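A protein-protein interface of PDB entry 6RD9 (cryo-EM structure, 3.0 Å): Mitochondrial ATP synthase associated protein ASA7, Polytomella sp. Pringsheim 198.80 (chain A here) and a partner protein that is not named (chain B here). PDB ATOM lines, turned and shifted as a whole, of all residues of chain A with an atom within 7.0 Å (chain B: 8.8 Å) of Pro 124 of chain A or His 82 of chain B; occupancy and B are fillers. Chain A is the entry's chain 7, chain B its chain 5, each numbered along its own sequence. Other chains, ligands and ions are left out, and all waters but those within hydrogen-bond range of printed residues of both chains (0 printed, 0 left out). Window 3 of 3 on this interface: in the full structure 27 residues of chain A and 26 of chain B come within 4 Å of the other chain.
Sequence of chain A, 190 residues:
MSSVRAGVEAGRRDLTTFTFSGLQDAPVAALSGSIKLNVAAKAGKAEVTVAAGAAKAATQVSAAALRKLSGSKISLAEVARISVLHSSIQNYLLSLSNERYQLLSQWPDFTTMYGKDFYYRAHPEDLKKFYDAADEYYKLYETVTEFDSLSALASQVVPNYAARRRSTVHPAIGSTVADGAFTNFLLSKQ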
ATOM      1  N   TYR A 119     -22.105  -6.956  -6.723  1.00  0.00           N
ATOM      2  CA  TYR A 119     -21.280  -8.115  -7.031  1.00  0.00           C
ATOM      3  C   TYR A 119     -20.604  -8.635  -5.784  1.00  0.00           C
ATOM      4  O   TYR A 119     -20.526  -9.844  -5.564  1.00  0.00           O
ATOM      5  CB  TYR A 119     -20.236  -7.739  -8.080  1.00  0.00           C
ATOM      6  CG  TYR A 119     -19.421  -8.861  -8.670  1.00  0.00           C
ATOM      7  CD1 TYR A 119     -18.345  -9.394  -8.000  1.00  0.00           C
ATOM      8  CD2 TYR A 119     -19.683  -9.335  -9.927  1.00  0.00           C
ATOM      9  CE1 TYR A 119     -17.605 -10.385  -8.525  1.00  0.00           C
ATOM     10  CE2 TYR A 119     -18.943 -10.345 -10.461  1.00  0.00           C
ATOM     11  CZ  TYR A 119     -17.902 -10.853  -9.749  1.00  0.00           C
ATOM     12  OH  TYR A 119     -17.134 -11.842 -10.258  1.00  0.00           O
ATOM     13  N   TYR A 120     -20.061  -7.738  -4.985  1.00  0.00           N
ATOM     14  CA  TYR A 120     -19.206  -8.104  -3.879  1.00  0.00           C
ATOM     15  C   TYR A 120     -19.938  -8.184  -2.564  1.00  0.00           C
ATOM     16  O   TYR A 120     -19.397  -8.727  -1.606  1.00  0.00           O
ATOM     17  CB  TYR A 120     -18.063  -7.117  -3.776  1.00  0.00           C
ATOM     18  CG  TYR A 120     -17.053  -7.335  -4.837  1.00  0.00           C
ATOM     19  CD1 TYR A 120     -16.431  -8.553  -4.972  1.00  0.00           C
ATOM     20  CD2 TYR A 120     -16.720  -6.336  -5.705  1.00  0.00           C
ATOM     21  CE1 TYR A 120     -15.516  -8.764  -5.948  1.00  0.00           C
ATOM     22  CE2 TYR A 120     -15.803  -6.534  -6.682  1.00  0.00           C
ATOM     23  CZ  TYR A 120     -15.199  -7.745  -6.795  1.00  0.00           C
ATOM     24  OH  TYR A 120     -14.280  -7.927  -7.785  1.00  0.00           O
ATOM     25  N   ALA A 122     -22.765  -9.837  -2.469  1.00  0.00           N
ATOM     26  CA  ALA A 122     -23.649 -10.969  -2.652  1.00  0.00           C
ATOM     27  C   ALA A 122     -22.891 -12.274  -2.578  1.00  0.00           C
ATOM     28  O   ALA A 122     -21.709 -12.342  -2.906  1.00  0.00           O
ATOM     29  CB  ALA A 122     -24.360 -10.892  -3.992  1.00  0.00           C
ATOM     30  N   HIS A 123     -23.604 -13.297  -2.142  1.00  0.00           N
ATOM     31  CA  HIS A 123     -23.107 -14.655  -2.097  1.00  0.00           C
ATOM     32  C   HIS A 123     -22.687 -15.081  -3.492  1.00  0.00           C
ATOM     33  O   HIS A 123     -23.372 -14.758  -4.459  1.00  0.00           O
ATOM     34  CB  HIS A 123     -24.220 -15.554  -1.580  1.00  0.00           C
ATOM     35  CG  HIS A 123     -23.807 -16.942  -1.241  1.00  0.00           C
ATOM     36  ND1 HIS A 123     -23.934 -17.455   0.024  1.00  0.00           N
ATOM     37  CD2 HIS A 123     -23.360 -17.954  -2.012  1.00  0.00           C
ATOM     38  CE1 HIS A 123     -23.538 -18.712   0.026  1.00  0.00           C
ATOM     39  NE2 HIS A 123     -23.177 -19.036  -1.198  1.00  0.00           N
ATOM     40  N   PRO A 124     -21.554 -15.762  -3.639  1.00  0.00           N
ATOM     41  CA  PRO A 124     -21.073 -16.113  -4.981  1.00  0.00           C
ATOM     42  C   PRO A 124     -21.963 -17.060  -5.752  1.00  0.00           C
ATOM     43  O   PRO A 124     -21.816 -17.164  -6.966  1.00  0.00           O
ATOM     44  CB  PRO A 124     -19.717 -16.750  -4.689  1.00  0.00           C
ATOM     45  CG  PRO A 124     -19.313 -16.151  -3.438  1.00  0.00           C
ATOM     46  CD  PRO A 124     -20.517 -15.965  -2.628  1.00  0.00           C
ATOM     47  N   GLU A 125     -22.866 -17.766  -5.090  1.00  0.00           N
ATOM     48  CA  GLU A 125     -23.805 -18.632  -5.781  1.00  0.00           C
ATOM     49  C   GLU A 125     -25.124 -17.945  -6.064  1.00  0.00           C
ATOM     50  O   GLU A 125     -25.827 -18.336  -6.993  1.00  0.00           O
ATOM     51  CB  GLU A 125     -24.042 -19.893  -4.971  1.00  0.00           C
ATOM     52  CG  GLU A 125     -22.811 -20.740  -4.853  1.00  0.00           C
ATOM     53  CD  GLU A 125     -22.369 -21.308  -6.184  1.00  0.00           C
ATOM     54  OE1 GLU A 125     -23.238 -21.607  -7.027  1.00  0.00           O
ATOM     55  OE2 GLU A 125     -21.149 -21.457  -6.392  1.00  0.00           O
ATOM     56  N   ASP A 126     -25.497 -16.956  -5.263  1.00  0.00           N
ATOM     57  CA  ASP A 126     -26.664 -16.149  -5.562  1.00  0.00           C
ATOM     58  C   ASP A 126     -26.362 -15.074  -6.570  1.00  0.00           C
ATOM     59  O   ASP A 126     -27.280 -14.395  -7.017  1.00  0.00           O
ATOM     60  CB  ASP A 126     -27.204 -15.492  -4.308  1.00  0.00           C
ATOM     61  CG  ASP A 126     -27.659 -16.484  -3.306  1.00  0.00           C
ATOM     62  OD1 ASP A 126     -27.794 -17.662  -3.671  1.00  0.00           O
ATOM     63  OD2 ASP A 126     -27.883 -16.093  -2.147  1.00  0.00           O
ATOM     64  N   LEU A 127     -25.103 -14.853  -6.886  1.00  0.00           N
ATOM     65  CA  LEU A 127     -24.776 -13.966  -7.982  1.00  0.00           C
ATOM     66  C   LEU A 127     -24.712 -14.722  -9.292  1.00  0.00           C
ATOM     67  O   LEU A 127     -25.057 -14.176 -10.336  1.00  0.00           O
ATOM     68  CB  LEU A 127     -23.449 -13.290  -7.723  1.00  0.00           C
ATOM     69  CG  LEU A 127     -23.170 -12.172  -8.687  1.00  0.00           C
ATOM     70  CD1 LEU A 127     -23.896 -10.936  -8.261  1.00  0.00           C
ATOM     71  CD2 LEU A 127     -21.732 -11.992  -8.795  1.00  0.00           C
ATOM     72  N   LYS A 128     -24.277 -15.973  -9.268  1.00  0.00           N
ATOM     73  CA  LYS A 128     -24.302 -16.764 -10.485  1.00  0.00           C
ATOM     74  C   LYS A 128     -25.716 -17.149 -10.864  1.00  0.00           C
ATOM     75  O   LYS A 128     -25.993 -17.376 -12.039  1.00  0.00           O
ATOM     76  CB  LYS A 128     -23.455 -18.012 -10.327  1.00  0.00           C
ATOM     77  CG  LYS A 128     -22.002 -17.715 -10.167  1.00  0.00           C
ATOM     78  CD  LYS A 128     -21.180 -18.960 -10.328  1.00  0.00           C
ATOM     79  CE  LYS A 128     -19.745 -18.682  -9.991  1.00  0.00           C
ATOM     80  NZ  LYS A 128     -19.615 -18.373  -8.552  1.00  0.00           N
ATOM     81  N   LYS A 129     -26.618 -17.249  -9.894  1.00  0.00           N
ATOM     82  CA  LYS A 129     -28.014 -17.444 -10.238  1.00  0.00           C
ATOM     83  C   LYS A 129     -28.612 -16.183 -10.814  1.00  0.00           C
ATOM     84  O   LYS A 129     -29.440 -16.253 -11.717  1.00  0.00           O
ATOM     85  CB  LYS A 129     -28.806 -17.889  -9.020  1.00  0.00           C
ATOM     86  CG  LYS A 129     -28.598 -19.326  -8.684  1.00  0.00           C
ATOM     87  CD  LYS A 129     -29.175 -19.673  -7.346  1.00  0.00           C
ATOM     88  CE  LYS A 129     -28.770 -21.076  -6.966  1.00  0.00           C
ATOM     89  NZ  LYS A 129     -28.981 -21.343  -5.527  1.00  0.00           N
ATOM     90  N   GLN B  75      -5.676 -18.517  -5.240  1.00  0.00           N
ATOM     91  CA  GLN B  75      -6.956 -18.761  -4.600  1.00  0.00           C
ATOM     92  C   GLN B  75      -7.615 -17.493  -4.105  1.00  0.00           C
ATOM     93  O   GLN B  75      -8.792 -17.524  -3.762  1.00  0.00           O
ATOM     94  CB  GLN B  75      -6.786 -19.704  -3.432  1.00  0.00           C
ATOM     95  CG  GLN B  75      -6.208 -21.017  -3.817  1.00  0.00           C
ATOM     96  CD  GLN B  75      -6.301 -22.011  -2.710  1.00  0.00           C
ATOM     97  OE1 GLN B  75      -6.609 -21.666  -1.585  1.00  0.00           O
ATOM     98  NE2 GLN B  75      -6.066 -23.264  -3.027  1.00  0.00           N
ATOM     99  N   VAL B  76      -6.880 -16.397  -4.006  1.00  0.00           N
ATOM    100  CA  VAL B  76      -7.521 -15.118  -3.767  1.00  0.00           C
ATOM    101  C   VAL B  76      -8.153 -14.619  -5.045  1.00  0.00           C
ATOM    102  O   VAL B  76      -9.319 -14.225  -5.061  1.00  0.00           O
ATOM    103  CB  VAL B  76      -6.504 -14.119  -3.204  1.00  0.00           C
ATOM    104  CG1 VAL B  76      -7.103 -12.772  -3.085  1.00  0.00           C
ATOM    105  CG2 VAL B  76      -6.096 -14.563  -1.884  1.00  0.00           C
ATOM    106  N   LEU B  77      -7.415 -14.677  -6.146  1.00  0.00           N
ATOM    107  CA  LEU B  77      -7.888 -14.155  -7.413  1.00  0.00           C
ATOM    108  C   LEU B  77      -8.992 -14.984  -8.027  1.00  0.00           C
ATOM    109  O   LEU B  77      -9.601 -14.543  -8.999  1.00  0.00           O
ATOM    110  CB  LEU B  77      -6.747 -14.079  -8.407  1.00  0.00           C
ATOM    111  CG  LEU B  77      -5.691 -13.025  -8.185  1.00  0.00           C
ATOM    112  CD1 LEU B  77      -4.852 -12.983  -9.410  1.00  0.00           C
ATOM    113  CD2 LEU B  77      -6.326 -11.702  -7.936  1.00  0.00           C
ATOM    114  N   GLU B  78      -9.240 -16.183  -7.535  1.00  0.00           N
ATOM    115  CA  GLU B  78     -10.374 -16.939  -8.018  1.00  0.00           C
ATOM    116  C   GLU B  78     -11.543 -16.924  -7.057  1.00  0.00           C
ATOM    117  O   GLU B  78     -12.614 -17.409  -7.414  1.00  0.00           O
ATOM    118  CB  GLU B  78      -9.965 -18.373  -8.307  1.00  0.00           C
ATOM    119  CG  GLU B  78      -9.840 -19.235  -7.110  1.00  0.00           C
ATOM    120  CD  GLU B  78      -9.317 -20.593  -7.474  1.00  0.00           C
ATOM    121  OE1 GLU B  78      -9.005 -20.799  -8.666  1.00  0.00           O
ATOM    122  OE2 GLU B  78      -9.206 -21.450  -6.574  1.00  0.00           O
ATOM    123  N   ASN B  79     -11.370 -16.387  -5.861  1.00  0.00           N
ATOM    124  CA  ASN B  79     -12.463 -16.198  -4.928  1.00  0.00           C
ATOM    125  C   ASN B  79     -12.934 -14.764  -4.891  1.00  0.00           C
ATOM    126  O   ASN B  79     -14.034 -14.502  -4.410  1.00  0.00           O
ATOM    127  CB  ASN B  79     -12.053 -16.608  -3.515  1.00  0.00           C
ATOM    128  CG  ASN B  79     -12.082 -18.086  -3.301  1.00  0.00           C
ATOM    129  OD1 ASN B  79     -12.910 -18.595  -2.563  1.00  0.00           O
ATOM    130  ND2 ASN B  79     -11.176 -18.788  -3.941  1.00  0.00           N
ATOM    131  N   VAL B  80     -12.115 -13.834  -5.350  1.00  0.00           N
ATOM    132  CA  VAL B  80     -12.510 -12.441  -5.441  1.00  0.00           C
ATOM    133  C   VAL B  80     -13.088 -12.139  -6.816  1.00  0.00           C
ATOM    134  O   VAL B  80     -14.076 -11.414  -6.932  1.00  0.00           O
ATOM    135  CB  VAL B  80     -11.285 -11.574  -5.110  1.00  0.00           C
ATOM    136  CG1 VAL B  80     -11.397 -10.189  -5.646  1.00  0.00           C
ATOM    137  CG2 VAL B  80     -11.093 -11.533  -3.631  1.00  0.00           C
ATOM    138  N   PHE B  81     -12.563 -12.772  -7.847  1.00  0.00           N
ATOM    139  CA  PHE B  81     -12.989 -12.570  -9.215  1.00  0.00           C
ATOM    140  C   PHE B  81     -13.678 -13.822  -9.707  1.00  0.00           C
ATOM    141  O   PHE B  81     -13.270 -14.397 -10.716  1.00  0.00           O
ATOM    142  CB  PHE B  81     -11.801 -12.235 -10.093  1.00  0.00           C
ATOM    143  CG  PHE B  81     -11.110 -10.982  -9.704  1.00  0.00           C
ATOM    144  CD1 PHE B  81     -11.832  -9.868  -9.342  1.00  0.00           C
ATOM    145  CD2 PHE B  81      -9.741 -10.909  -9.713  1.00  0.00           C
ATOM    146  CE1 PHE B  81     -11.205  -8.714  -8.988  1.00  0.00           C
ATOM    147  CE2 PHE B  81      -9.111  -9.756  -9.356  1.00  0.00           C
ATOM    148  CZ  PHE B  81      -9.847  -8.661  -8.995  1.00  0.00           C
ATOM    149  N   HIS B  82     -14.672 -14.288  -8.955  1.00  0.00           N
ATOM    150  CA  HIS B  82     -15.252 -15.602  -9.196  1.00  0.00           C
ATOM    151  C   HIS B  82     -16.051 -15.664 -10.492  1.00  0.00           C
ATOM    152  O   HIS B  82     -15.977 -16.661 -11.215  1.00  0.00           O
ATOM    153  CB  HIS B  82     -16.116 -16.004  -8.011  1.00  0.00           C
ATOM    154  CG  HIS B  82     -17.026 -14.929  -7.518  1.00  0.00           C
ATOM    155  ND1 HIS B  82     -18.326 -14.800  -7.949  1.00  0.00           N
ATOM    156  CD2 HIS B  82     -16.838 -13.953  -6.605  1.00  0.00           C
ATOM    157  CE1 HIS B  82     -18.895 -13.783  -7.329  1.00  0.00           C
ATOM    158  NE2 HIS B  82     -18.012 -13.251  -6.509  1.00  0.00           N
ATOM    159  N   THR B  83     -16.819 -14.630 -10.806  1.00  0.00           N
ATOM    160  CA  THR B  83     -17.693 -14.620 -11.971  1.00  0.00           C
ATOM    161  C   THR B  83     -17.261 -13.495 -12.891  1.00  0.00           C
ATOM    162  O   THR B  83     -16.923 -12.410 -12.423  1.00  0.00           O
ATOM    163  CB  THR B  83     -19.160 -14.420 -11.556  1.00  0.00           C
ATOM    164  OG1 THR B  83     -19.468 -15.283 -10.461  1.00  0.00           O
ATOM    165  CG2 THR B  83     -20.100 -14.761 -12.676  1.00  0.00           C
ATOM    166  N   ALA B  84     -17.255 -13.752 -14.184  1.00  0.00           N
ATOM    167  CA  ALA B  84     -16.970 -12.701 -15.150  1.00  0.00           C
ATOM    168  C   ALA B  84     -18.107 -11.698 -15.147  1.00  0.00           C
ATOM    169  O   ALA B  84     -19.246 -12.079 -15.426  1.00  0.00           O
ATOM    170  CB  ALA B  84     -16.798 -13.287 -16.536  1.00  0.00           C
ATOM    171  N   PRO B  85     -17.857 -10.429 -14.857  1.00  0.00           N
ATOM    172  CA  PRO B  85     -18.953  -9.491 -14.616  1.00  0.00           C
ATOM    173  C   PRO B  85     -19.669  -9.099 -15.899  1.00  0.00           C
ATOM    174  O   PRO B  85     -19.120  -9.153 -16.998  1.00  0.00           O
ATOM    175  CB  PRO B  85     -18.244  -8.289 -13.992  1.00  0.00           C
ATOM    176  CG  PRO B  85     -16.918  -8.323 -14.590  1.00  0.00           C
ATOM    177  CD  PRO B  85     -16.553  -9.765 -14.780  1.00  0.00           C
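The backbone NH of Thr 83 of chain B lies within hydrogen-bond range of the side-chain hydroxyl of Tyr 119 of chain A (2.9 Å).
ND1 of His 82 of chain B is in hydrogen-bond range of OG1 of Thr 83 of chain B (2.8 Å).
The side-chain amino group (NZ) of Lys 128 of chain A sits at hydrogen-bond distance from the backbone carbonyl oxygen (O) of Pro 124 of chain A (3.0 Å).
Among the printed residues, pairs that only touch across the chains: Tyr 119 of chain A with His 82 of chain B, Tyr 120 of chain A with Val 80 of chain B, Tyr 120 of chain A with Phe 81 of chain B, Pro 124 of chain A with His 82 of chain B, Leu 127 of chain A with His 82 of chain B, Lys 128 of chain A with His 82 of chain B and Lys 128 of chain A with Thr 83 of chain B.
Of the printed residues of chain B, Pro 124 of chain A touches His 82 (3.96 Å).
His 82 of chain B touches four residues of chain A.
No residue of chain B comes within 4 Å of Glu 125 of chain A.
Of the printed residues of chain A, Thr 83 of chain B touches Tyr 119 (2.2 Å) and Lys 128 (3.4 Å).
Of the printed residues of chain B, Tyr 120 of chain A touches Val 80 (3.2 Å) and Phe 81 (3.4 Å).
Printed residues of chain A within 4 Å of Phe 81 of chain B: Tyr 120.
Leu 77 of chain B touches none of the printed residues of chain A.
The nearest residue of chain A that does not touch His 82 of chain B is Tyr 120 of chain A (5.2 Å).
The nearest printed residue of chain A that does not touch Thr 83 of chain B is Leu 127 of chain A (4.3 Å).
Of the 10 printed residues of chain A, 5 touch a printed residue of chain B.
Printed residues of chain A that touch a printed residue of chain B: Tyr 119, Tyr 120, Pro 124, Leu 127 and Lys 128.
Hydrophobic or aromatic side chains of chain A within 4 Å of the printed part of chain B: Tyr 119, Tyr 120 and Leu 127.
Printed residues of chain B that touch a printed residue of chain A: Val 80, Phe 81, His 82 and Thr 83.
Hydrophobic or aromatic side chains of chain B within 4 Å of the printed part of chain A: Phe 81 and His 82.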
